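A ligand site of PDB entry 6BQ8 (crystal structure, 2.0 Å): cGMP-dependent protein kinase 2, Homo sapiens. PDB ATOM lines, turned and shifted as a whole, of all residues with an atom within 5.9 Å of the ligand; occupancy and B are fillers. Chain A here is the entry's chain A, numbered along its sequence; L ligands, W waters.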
ATOM      1  N   ILE A  48      -2.416 -11.440 -19.534  1.00  0.00           N
ATOM      2  CA  ILE A  48      -3.244 -12.626 -19.329  1.00  0.00           C
ATOM      3  C   ILE A  48      -2.688 -13.398 -18.146  1.00  0.00           C
ATOM      4  O   ILE A  48      -1.472 -13.567 -18.032  1.00  0.00           O
ATOM      5  CB  ILE A  48      -3.206 -13.567 -20.560  1.00  0.00           C
ATOM      6  CG1 ILE A  48      -3.963 -12.959 -21.741  1.00  0.00           C
ATOM      7  CG2 ILE A  48      -3.792 -14.933 -20.198  1.00  0.00           C
ATOM      8  CD1 ILE A  48      -3.894 -13.800 -22.999  1.00  0.00           C
ATOM      9  N   THR A  56     -11.092 -12.922 -25.185  1.00  0.00           N
ATOM     10  CA  THR A  56     -10.535 -11.991 -26.159  1.00  0.00           C
ATOM     11  C   THR A  56      -9.264 -12.518 -26.826  1.00  0.00           C
ATOM     12  O   THR A  56      -8.512 -13.314 -26.249  1.00  0.00           O
ATOM     13  CB  THR A  56     -10.290 -10.633 -25.520  1.00  0.00           C
ATOM     14  OG1 THR A  56      -9.529 -10.776 -24.334  1.00  0.00           O
ATOM     15  CG2 THR A  56     -11.578  -9.890 -25.153  1.00  0.00           C
ATOM     16  N   VAL A  67       5.976 -15.399 -22.305  1.00  0.00           N
ATOM     17  CA  VAL A  67       4.953 -16.401 -22.049  1.00  0.00           C
ATOM     18  C   VAL A  67       5.493 -17.332 -20.965  1.00  0.00           C
ATOM     19  O   VAL A  67       6.536 -17.937 -21.144  1.00  0.00           O
ATOM     20  CB  VAL A  67       4.702 -17.222 -23.327  1.00  0.00           C
ATOM     21  CG1 VAL A  67       3.551 -18.212 -23.109  1.00  0.00           C
ATOM     22  CG2 VAL A  67       4.411 -16.303 -24.527  1.00  0.00           C
ATOM     23  N   GLN A  69       4.436 -20.484 -17.900  1.00  0.00           N
ATOM     24  CA  GLN A  69       3.455 -21.508 -17.601  1.00  0.00           C
ATOM     25  C   GLN A  69       3.868 -22.339 -16.387  1.00  0.00           C
ATOM     26  O   GLN A  69       5.042 -22.646 -16.217  1.00  0.00           O
ATOM     27  CB  GLN A  69       3.320 -22.403 -18.841  1.00  0.00           C
ATOM     28  CG  GLN A  69       2.182 -23.389 -18.829  1.00  0.00           C
ATOM     29  CD  GLN A  69       2.153 -24.216 -20.095  1.00  0.00           C
ATOM     30  OE1 GLN A  69       3.138 -24.865 -20.452  1.00  0.00           O
ATOM     31  NE2 GLN A  69       1.010 -24.214 -20.782  1.00  0.00           N
ATOM     32  N   ILE A  80       8.430 -20.046 -21.316  1.00  0.00           N
ATOM     33  CA  ILE A  80       8.227 -20.785 -22.555  1.00  0.00           C
ATOM     34  C   ILE A  80       8.763 -20.117 -23.816  1.00  0.00           C
ATOM     35  O   ILE A  80       9.382 -20.766 -24.656  1.00  0.00           O
ATOM     36  CB  ILE A  80       6.722 -21.037 -22.750  1.00  0.00           C
ATOM     37  CG1 ILE A  80       6.143 -21.736 -21.525  1.00  0.00           C
ATOM     38  CG2 ILE A  80       6.469 -21.845 -24.002  1.00  0.00           C
ATOM     39  CD1 ILE A  80       6.866 -23.019 -21.142  1.00  0.00           C
ATOM     40  N   LYS A  81       8.518 -18.823 -23.955  1.00  0.00           N
ATOM     41  CA  LYS A  81       9.000 -18.106 -25.127  1.00  0.00           C
ATOM     42  C   LYS A  81       8.675 -16.637 -25.029  1.00  0.00           C
ATOM     43  O   LYS A  81       8.066 -16.199 -24.060  1.00  0.00           O
ATOM     44  CB  LYS A  81       8.393 -18.681 -26.422  1.00  0.00           C
ATOM     45  CG  LYS A  81       6.868 -18.610 -26.508  1.00  0.00           C
ATOM     46  CD  LYS A  81       6.353 -18.981 -27.910  1.00  0.00           C
ATOM     47  CE  LYS A  81       6.411 -20.487 -28.202  1.00  0.00           C
ATOM     48  NZ  LYS A  81       5.313 -21.271 -27.562  1.00  0.00           N
ATOM     49  N   LEU A  83       7.275 -13.133 -27.386  1.00  0.00           N
ATOM     50  CA  LEU A  83       6.554 -12.747 -28.591  1.00  0.00           C
ATOM     51  C   LEU A  83       6.856 -11.295 -28.875  1.00  0.00           C
ATOM     52  O   LEU A  83       6.994 -10.489 -27.956  1.00  0.00           O
ATOM     53  CB  LEU A  83       5.043 -12.931 -28.425  1.00  0.00           C
ATOM     54  CG  LEU A  83       4.534 -14.355 -28.198  1.00  0.00           C
ATOM     55  CD1 LEU A  83       3.022 -14.351 -28.078  1.00  0.00           C
ATOM     56  CD2 LEU A  83       4.970 -15.276 -29.329  1.00  0.00           C
ATOM     57  N   TYR A  88       0.551 -12.829 -32.179  1.00  0.00           N
ATOM     58  CA  TYR A  88      -0.723 -12.811 -31.469  1.00  0.00           C
ATOM     59  C   TYR A  88      -0.823 -13.906 -30.407  1.00  0.00           C
ATOM     60  O   TYR A  88       0.032 -14.796 -30.331  1.00  0.00           O
ATOM     61  CB  TYR A  88      -1.865 -12.962 -32.471  1.00  0.00           C
ATOM     62  CG  TYR A  88      -1.674 -14.170 -33.371  1.00  0.00           C
ATOM     63  CD1 TYR A  88      -2.089 -15.434 -32.974  1.00  0.00           C
ATOM     64  CD2 TYR A  88      -1.046 -14.035 -34.620  1.00  0.00           C
ATOM     65  CE1 TYR A  88      -1.896 -16.533 -33.783  1.00  0.00           C
ATOM     66  CE2 TYR A  88      -0.843 -15.129 -35.446  1.00  0.00           C
ATOM     67  CZ  TYR A  88      -1.273 -16.380 -35.019  1.00  0.00           C
ATOM     68  OH  TYR A  88      -1.094 -17.489 -35.827  1.00  0.00           O
ATOM     69  N   PHE A  89      -1.877 -13.844 -29.600  1.00  0.00           N
ATOM     70  CA  PHE A  89      -2.076 -14.839 -28.560  1.00  0.00           C
ATOM     71  C   PHE A  89      -3.471 -14.757 -27.965  1.00  0.00           C
ATOM     72  O   PHE A  89      -4.198 -13.793 -28.207  1.00  0.00           O
ATOM     73  CB  PHE A  89      -0.997 -14.657 -27.478  1.00  0.00           C
ATOM     74  CG  PHE A  89      -0.910 -13.232 -26.929  1.00  0.00           C
ATOM     75  CD1 PHE A  89      -1.669 -12.862 -25.816  1.00  0.00           C
ATOM     76  CD2 PHE A  89      -0.080 -12.283 -27.519  1.00  0.00           C
ATOM     77  CE1 PHE A  89      -1.607 -11.581 -25.308  1.00  0.00           C
ATOM     78  CE2 PHE A  89      -0.007 -10.988 -27.024  1.00  0.00           C
ATOM     79  CZ  PHE A  89      -0.780 -10.639 -25.913  1.00  0.00           C
ATOM     80  N   GLY A  90      -3.852 -15.768 -27.205  1.00  0.00           N
ATOM     81  CA  GLY A  90      -5.170 -15.785 -26.591  1.00  0.00           C
ATOM     82  C   GLY A  90      -6.193 -16.563 -27.389  1.00  0.00           C
ATOM     83  O   GLY A  90      -7.329 -16.702 -26.949  1.00  0.00           O
ATOM     84  N   GLU A  91      -5.828 -17.078 -28.563  1.00  0.00           N
ATOM     85  CA  GLU A  91      -6.792 -17.827 -29.353  1.00  0.00           C
ATOM     86  C   GLU A  91      -7.133 -19.200 -28.749  1.00  0.00           C
ATOM     87  O   GLU A  91      -8.209 -19.744 -28.990  1.00  0.00           O
ATOM     88  CB  GLU A  91      -6.288 -18.033 -30.792  1.00  0.00           C
ATOM     89  CG  GLU A  91      -5.101 -18.996 -30.918  1.00  0.00           C
ATOM     90  CD  GLU A  91      -3.878 -18.551 -30.161  1.00  0.00           C
ATOM     91  OE1 GLU A  91      -3.447 -17.396 -30.349  1.00  0.00           O
ATOM     92  OE2 GLU A  91      -3.332 -19.354 -29.362  1.00  0.00           O
ATOM     93  N   LYS A  92      -6.206 -19.783 -28.010  1.00  0.00           N
ATOM     94  CA  LYS A  92      -6.431 -21.112 -27.456  1.00  0.00           C
ATOM     95  C   LYS A  92      -7.703 -21.217 -26.598  1.00  0.00           C
ATOM     96  O   LYS A  92      -8.465 -22.183 -26.714  1.00  0.00           O
ATOM     97  CB  LYS A  92      -5.216 -21.622 -26.693  1.00  0.00           C
ATOM     98  CG  LYS A  92      -5.252 -23.124 -26.465  1.00  0.00           C
ATOM     99  CD  LYS A  92      -4.057 -23.595 -25.655  1.00  0.00           C
ATOM    100  CE  LYS A  92      -3.955 -25.123 -25.640  1.00  0.00           C
ATOM    101  NZ  LYS A  92      -5.218 -25.792 -25.188  1.00  0.00           N
ATOM    102  N   ALA A  93      -7.914 -20.224 -25.744  1.00  0.00           N
ATOM    103  CA  ALA A  93      -9.095 -20.239 -24.879  1.00  0.00           C
ATOM    104  C   ALA A  93     -10.393 -20.283 -25.696  1.00  0.00           C
ATOM    105  O   ALA A  93     -11.380 -20.906 -25.270  1.00  0.00           O
ATOM    106  CB  ALA A  93      -9.072 -19.031 -23.947  1.00  0.00           C
ATOM    107  N   LEU A  94     -10.406 -19.600 -26.839  1.00  0.00           N
ATOM    108  CA  LEU A  94     -11.602 -19.549 -27.666  1.00  0.00           C
ATOM    109  C   LEU A  94     -11.832 -20.835 -28.456  1.00  0.00           C
ATOM    110  O   LEU A  94     -12.979 -21.255 -28.659  1.00  0.00           O
ATOM    111  CB  LEU A  94     -11.519 -18.357 -28.628  1.00  0.00           C
ATOM    112  CG  LEU A  94     -11.069 -17.016 -28.050  1.00  0.00           C
ATOM    113  CD1 LEU A  94     -11.256 -15.941 -29.099  1.00  0.00           C
ATOM    114  CD2 LEU A  94     -11.806 -16.641 -26.767  1.00  0.00           C
ATOM    115  N   VAL A  99     -10.150 -22.047 -19.853  1.00  0.00           N
ATOM    116  CA  VAL A  99      -9.561 -20.882 -19.202  1.00  0.00           C
ATOM    117  C   VAL A  99      -8.184 -20.643 -19.794  1.00  0.00           C
ATOM    118  O   VAL A  99      -7.656 -21.515 -20.497  1.00  0.00           O
ATOM    119  CB  VAL A  99      -9.477 -21.090 -17.674  1.00  0.00           C
ATOM    120  CG1 VAL A  99     -10.866 -21.282 -17.065  1.00  0.00           C
ATOM    121  CG2 VAL A  99      -8.556 -22.263 -17.323  1.00  0.00           C
ATOM    122  N   ARG A 100      -7.596 -19.482 -19.515  1.00  0.00           N
ATOM    123  CA  ARG A 100      -6.276 -19.142 -20.019  1.00  0.00           C
ATOM    124  C   ARG A 100      -5.284 -20.196 -19.533  1.00  0.00           C
ATOM    125  O   ARG A 100      -5.335 -20.602 -18.379  1.00  0.00           O
ATOM    126  CB  ARG A 100      -5.861 -17.739 -19.589  1.00  0.00           C
ATOM    127  CG  ARG A 100      -6.855 -16.678 -20.027  1.00  0.00           C
ATOM    128  CD  ARG A 100      -6.906 -16.562 -21.558  1.00  0.00           C
ATOM    129  NE  ARG A 100      -7.494 -15.287 -21.958  1.00  0.00           N
ATOM    130  CZ  ARG A 100      -7.729 -14.904 -23.207  1.00  0.00           C
ATOM    131  NH1 ARG A 100      -7.426 -15.688 -24.225  1.00  0.00           N
ATOM    132  NH2 ARG A 100      -8.279 -13.713 -23.450  1.00  0.00           N
ATOM    133  N   SER A 101      -4.450 -20.684 -20.442  1.00  0.00           N
ATOM    134  CA  SER A 101      -3.538 -21.772 -20.133  1.00  0.00           C
ATOM    135  C   SER A 101      -2.088 -21.378 -19.922  1.00  0.00           C
ATOM    136  O   SER A 101      -1.226 -22.237 -19.809  1.00  0.00           O
ATOM    137  CB  SER A 101      -3.618 -22.826 -21.249  1.00  0.00           C
ATOM    138  OG  SER A 101      -3.225 -22.245 -22.487  1.00  0.00           O
ATOM    139  N   ALA A 102      -1.824 -20.069 -19.870  1.00  0.00           N
ATOM    140  CA  ALA A 102      -0.486 -19.566 -19.674  1.00  0.00           C
ATOM    141  C   ALA A 102      -0.538 -18.083 -19.337  1.00  0.00           C
ATOM    142  O   ALA A 102      -1.550 -17.422 -19.591  1.00  0.00           O
ATOM    143  CB  ALA A 102       0.340 -19.780 -20.945  1.00  0.00           C
ATOM    144  N   ASN A 103       0.555 -17.552 -18.778  1.00  0.00           N
ATOM    145  CA  ASN A 103       0.639 -16.133 -18.435  1.00  0.00           C
ATOM    146  C   ASN A 103       1.283 -15.428 -19.608  1.00  0.00           C
ATOM    147  O   ASN A 103       2.201 -15.964 -20.227  1.00  0.00           O
ATOM    148  CB  ASN A 103       1.547 -15.893 -17.215  1.00  0.00           C
ATOM    149  CG  ASN A 103       1.100 -16.660 -15.975  1.00  0.00           C
ATOM    150  OD1 ASN A 103       0.070 -16.361 -15.391  1.00  0.00           O
ATOM    151  ND2 ASN A 103       1.880 -17.682 -15.597  1.00  0.00           N
ATOM    152  N   ILE A 104       0.859 -14.194 -19.859  1.00  0.00           N
ATOM    153  CA  ILE A 104       1.466 -13.371 -20.892  1.00  0.00           C
ATOM    154  C   ILE A 104       1.812 -12.115 -20.112  1.00  0.00           C
ATOM    155  O   ILE A 104       0.941 -11.453 -19.540  1.00  0.00           O
ATOM    156  CB  ILE A 104       0.503 -13.046 -22.056  1.00  0.00           C
ATOM    157  CG1 ILE A 104      -0.031 -14.347 -22.698  1.00  0.00           C
ATOM    158  CG2 ILE A 104       1.215 -12.151 -23.090  1.00  0.00           C
ATOM    159  CD1 ILE A 104       1.023 -15.153 -23.474  1.00  0.00           C
ATOM    160  N   TYR A 134      -6.293 -23.994 -39.758  1.00  0.00           N
ATOM    161  CA  TYR A 134      -4.910 -23.664 -39.425  1.00  0.00           C
ATOM    162  C   TYR A 134      -4.766 -23.494 -37.916  1.00  0.00           C
ATOM    163  O   TYR A 134      -3.829 -23.994 -37.294  1.00  0.00           O
ATOM    164  CB  TYR A 134      -4.477 -22.382 -40.117  1.00  0.00           C
ATOM    165  CG  TYR A 134      -3.129 -21.871 -39.649  1.00  0.00           C
ATOM    166  CD1 TYR A 134      -1.953 -22.540 -39.980  1.00  0.00           C
ATOM    167  CD2 TYR A 134      -3.035 -20.723 -38.882  1.00  0.00           C
ATOM    168  CE1 TYR A 134      -0.720 -22.080 -39.547  1.00  0.00           C
ATOM    169  CE2 TYR A 134      -1.816 -20.254 -38.442  1.00  0.00           C
ATOM    170  CZ  TYR A 134      -0.663 -20.922 -38.775  1.00  0.00           C
ATOM    171  OH  TYR A 134       0.553 -20.430 -38.344  1.00  0.00           O
ATOM    172  N   LEU A 135      -5.716 -22.758 -37.348  1.00  0.00           N
ATOM    173  CA  LEU A 135      -5.743 -22.473 -35.912  1.00  0.00           C
ATOM    174  C   LEU A 135      -5.966 -23.711 -35.045  1.00  0.00           C
ATOM    175  O   LEU A 135      -5.395 -23.823 -33.966  1.00  0.00           O
ATOM    176  CB  LEU A 135      -6.811 -21.416 -35.641  1.00  0.00           C
ATOM    177  CG  LEU A 135      -6.339 -20.005 -35.247  1.00  0.00           C
ATOM    178  CD1 LEU A 135      -5.068 -19.570 -35.946  1.00  0.00           C
ATOM    179  CD2 LEU A 135      -7.460 -18.998 -35.475  1.00  0.00           C
ATOM    180  N   TYR A 138      -2.795 -25.650 -35.051  1.00  0.00           N
ATOM    181  CA  TYR A 138      -1.825 -25.016 -34.179  1.00  0.00           C
ATOM    182  C   TYR A 138      -2.169 -25.257 -32.703  1.00  0.00           C
ATOM    183  O   TYR A 138      -1.283 -25.521 -31.880  1.00  0.00           O
ATOM    184  CB  TYR A 138      -1.673 -23.533 -34.497  1.00  0.00           C
ATOM    185  CG  TYR A 138      -0.208 -23.114 -34.533  1.00  0.00           C
ATOM    186  CD1 TYR A 138       0.262 -22.218 -35.485  1.00  0.00           C
ATOM    187  CD2 TYR A 138       0.702 -23.659 -33.627  1.00  0.00           C
ATOM    188  CE1 TYR A 138       1.613 -21.869 -35.525  1.00  0.00           C
ATOM    189  CE2 TYR A 138       2.043 -23.325 -33.653  1.00  0.00           C
ATOM    190  CZ  TYR A 138       2.499 -22.430 -34.602  1.00  0.00           C
ATOM    191  OH  TYR A 138       3.826 -22.106 -34.627  1.00  0.00           O
ATOM    192  N   LEU A 142      -0.041 -27.118 -29.557  1.00  0.00           N
ATOM    193  CA  LEU A 142       0.181 -26.512 -28.246  1.00  0.00           C
ATOM    194  C   LEU A 142      -0.187 -27.471 -27.141  1.00  0.00           C
ATOM    195  O   LEU A 142       0.436 -27.474 -26.084  1.00  0.00           O
ATOM    196  CB  LEU A 142      -0.611 -25.215 -28.067  1.00  0.00           C
ATOM    197  CG  LEU A 142      -0.254 -24.024 -28.961  1.00  0.00           C
ATOM    198  CD1 LEU A 142      -0.988 -22.777 -28.486  1.00  0.00           C
ATOM    199  CD2 LEU A 142       1.250 -23.797 -28.977  1.00  0.00           C
ATOM    200  N   ASP A 145       2.694 -29.704 -26.776  1.00  0.00           N
ATOM    201  CA  ASP A 145       3.847 -29.083 -26.133  1.00  0.00           C
ATOM    202  C   ASP A 145       3.600 -29.000 -24.632  1.00  0.00           C
ATOM    203  O   ASP A 145       4.520 -29.216 -23.836  1.00  0.00           O
ATOM    204  CB  ASP A 145       4.137 -27.698 -26.705  1.00  0.00           C
ATOM    205  CG  ASP A 145       4.575 -27.752 -28.167  1.00  0.00           C
ATOM    206  OD1 ASP A 145       4.959 -28.852 -28.634  1.00  0.00           O
ATOM    207  OD2 ASP A 145       4.561 -26.691 -28.828  1.00  0.00           O
ATOM    208  N   ASP A 146       2.371 -28.707 -24.253  1.00  0.00           N
ATOM    209  CA  ASP A 146       2.001 -28.605 -22.857  1.00  0.00           C
ATOM    210  C   ASP A 146       2.221 -29.934 -22.167  1.00  0.00           C
ATOM    211  O   ASP A 146       2.829 -30.002 -21.101  1.00  0.00           O
ATOM    212  CB  ASP A 146       0.524 -28.224 -22.712  1.00  0.00           C
ATOM    213  CG  ASP A 146       0.262 -26.769 -23.022  1.00  0.00           C
ATOM    214  OD1 ASP A 146       1.239 -26.033 -23.293  1.00  0.00           O
ATOM    215  OD2 ASP A 146      -0.916 -26.362 -22.989  1.00  0.00           O
ATOM    216  N   ARG A 149       6.039 -30.727 -21.610  1.00  0.00           N
ATOM    217  CA  ARG A 149       6.701 -30.039 -20.503  1.00  0.00           C
ATOM    218  C   ARG A 149       5.959 -30.228 -19.169  1.00  0.00           C
ATOM    219  O   ARG A 149       6.357 -29.670 -18.147  1.00  0.00           O
ATOM    220  CB  ARG A 149       6.901 -28.561 -20.805  1.00  0.00           C
ATOM    221  CG  ARG A 149       5.631 -27.736 -20.777  1.00  0.00           C
ATOM    222  CD  ARG A 149       5.967 -26.273 -20.953  1.00  0.00           C
ATOM    223  NE  ARG A 149       6.302 -25.945 -22.328  1.00  0.00           N
ATOM    224  CZ  ARG A 149       5.406 -25.717 -23.286  1.00  0.00           C
ATOM    225  NH1 ARG A 149       4.108 -25.695 -23.008  1.00  0.00           N
ATOM    226  NH2 ARG A 149       5.812 -25.469 -24.520  1.00  0.00           N
HETATM  227  C1  LIG L   1       2.162 -23.024 -25.292  1.00  0.00           C
HETATM  228  N1  LIG L   1       1.179 -23.656 -24.566  1.00  0.00           N
HETATM  229  C2  LIG L   1      -0.028 -23.014 -24.249  1.00  0.00           C
HETATM  230  C3  LIG L   1       2.007 -19.535 -26.651  1.00  0.00           C
HETATM  231  C4  LIG L   1       0.489 -17.707 -29.510  1.00  0.00           C
HETATM  232  C5  LIG L   1      -0.206 -18.078 -30.673  1.00  0.00           C
HETATM  233  C6  LIG L   1       0.191 -19.270 -31.336  1.00  0.00           C
HETATM  234  C7  LIG L   1       1.930 -19.686 -29.682  1.00  0.00           C
HETATM  235 CL1  LIG L   1      -0.624 -19.806 -32.807  1.00  0.00          CL
HETATM  236  P1  LIG L   1      -4.666 -18.818 -24.027  1.00  0.00           P
HETATM  237  C8  LIG L   1      -2.433 -18.089 -22.945  1.00  0.00           C
HETATM  238  C9  LIG L   1      -1.785 -18.093 -24.291  1.00  0.00           C
HETATM  239  C10 LIG L   1      -2.439 -19.090 -25.212  1.00  0.00           C
HETATM  240  C11 LIG L   1      -1.629 -19.044 -26.483  1.00  0.00           C
HETATM  241  C12 LIG L   1      -0.268 -18.613 -25.873  1.00  0.00           C
HETATM  242  O1  LIG L   1      -0.414 -18.420 -24.438  1.00  0.00           O
HETATM  243  N2  LIG L   1       0.763 -19.673 -25.976  1.00  0.00           N
HETATM  244  C13 LIG L   1       0.708 -20.996 -25.414  1.00  0.00           C
HETATM  245  C14 LIG L   1       1.935 -21.620 -25.762  1.00  0.00           C
HETATM  246  O2  LIG L   1       3.348 -23.621 -25.621  1.00  0.00           O
HETATM  247  N3  LIG L   1      -0.278 -21.595 -24.694  1.00  0.00           N
HETATM  248  N4  LIG L   1      -1.056 -23.670 -23.510  1.00  0.00           N
HETATM  249  N5  LIG L   1       2.766 -20.706 -26.528  1.00  0.00           N
HETATM  250  S1  LIG L   1       2.498 -18.125 -27.514  1.00  0.00           S
HETATM  251  C15 LIG L   1       1.558 -18.508 -29.007  1.00  0.00           C
HETATM  252  C16 LIG L   1       1.261 -20.062 -30.830  1.00  0.00           C
HETATM  253  O3  LIG L   1      -2.007 -18.106 -27.480  1.00  0.00           O
HETATM  254  O4  LIG L   1      -3.847 -18.795 -25.443  1.00  0.00           O
HETATM  255  O5  LIG L   1      -6.040 -18.077 -24.335  1.00  0.00           O
HETATM  256  O6  LIG L   1      -3.906 -17.762 -23.134  1.00  0.00           O
HETATM  257  O7  LIG L   1      -4.734 -20.178 -23.327  1.00  0.00           O
HETATM  258  O   HOH W   1       5.176 -24.480 -27.609  1.00  0.00           O
HETATM  259  O   HOH W   2      -6.805 -21.878 -23.013  1.00  0.00           O
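The backbone NH (N) of Ala 93 lies within hydrogen-bond range of an oxygen (O5) of the ligand.
NH2 of Arg 149 is in hydrogen-bond range of O2 of the ligand (3.3 Å).
NH1 of Arg 100 lies within salt-bridge range of O5 of the ligand (2.8 Å).
NE2 of Gln 69 lies close to N4 of the ligand.
O3 of the ligand sits at hydrogen-bond distance from N of Gly 90 (3.0 Å).
An oxygen (O7) of the ligand sits at hydrogen-bond distance from the backbone NH (N) of Ser 101 (2.9 Å).
An oxygen (O3) of the ligand lies within hydrogen-bond range of the side-chain carboxylate (OE2) of Glu 91 (2.6 Å).
OD1 of Asp 146 is in hydrogen-bond range of N1 of the ligand.
The side-chain hydroxyl of Ser 101 is in hydrogen-bond range of an oxygen (O7) of the ligand.
NZ of Lys 81 sits at hydrogen-bond distance from N5 of the ligand.
The backbone carbonyl oxygen (O) of Lys 81 sits at hydrogen-bond distance from the backbone NH (N) of Val 67 (2.8 Å).
The guanidinium group (NH1) of Arg 100 lies within hydrogen-bond range of the backbone carbonyl oxygen (O) of Gly 90.
The backbone NH (N) of Ile 104 lies within hydrogen-bond range of the backbone carbonyl oxygen (O) of Ile 48.
O of Thr 56 sits at hydrogen-bond distance from NH2 of Arg 100, 2.8 Å away.
The side-chain carboxylate (OD1) of Asp 146 is in salt-bridge range of the guanidinium group (NH1) of Arg 149, at 2.9 Å.
OD1 of Asp 146 is in hydrogen-bond range of NE2 of Gln 69, 3.1 Å away.
The backbone carbonyl oxygen (O) of Val 67 sits at hydrogen-bond distance from the backbone NH (N) of Ile 80.
OE1 of Gln 69 lies within hydrogen-bond range of NH1 of Arg 149, 2.9 Å away.
Ile 48 touches the ligand.
Val 67 touches the ligand.
Ile 80 touches the ligand (CG2 to O2, 3.9 Å).
Leu 83 touches the ligand.
O of Tyr 88 touches C4 of the ligand, 3.1 Å away.
Phe 89 touches the ligand.
Lys 92 touches the ligand (CB to O4, 3.4 Å).
Ala 102 touches the ligand (O to C8, 3.5 Å).
Ile 104 touches the ligand.
Tyr 138 touches the ligand (CD1 to CL1, 3.7 Å).
CD2 of Leu 142 touches C1 of the ligand, at 3.9 Å.
Hydrophobic or aromatic side chains that line the ligand: Ile 48, Val 67, Ile 80, Leu 83, Tyr 88, Phe 89, Ala 93, Ala 102, Ile 104, Tyr 138 and Leu 142.
Within 4 Å of the ligand: Ile 48, Val 67, Gln 69, Ile 80, Lys 81, Leu 83, Tyr 88, Phe 89, Gly 90, Glu 91, Lys 92, Ala 93, Arg 100, Ser 101, Ala 102, Ile 104, Tyr 138, Leu 142, Asp 146 and Arg 149.
Water W2 lies within hydrogen-bond range of the backbone carbonyl oxygen (O) of Val 99 (2.7 Å), an oxygen (O7) of the ligand (2.7 Å) and the backbone NH (N) of Ala 93 (3.4 Å).
Water W1 lies within hydrogen-bond range of the side-chain carboxylate (OD2) of Asp 145 (2.6 Å), an oxygen (O2) of the ligand (2.8 Å), the side-chain amino group (NZ) of Lys 81 (3.2 Å) and the guanidinium group (NH2) of Arg 149 (3.3 Å).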
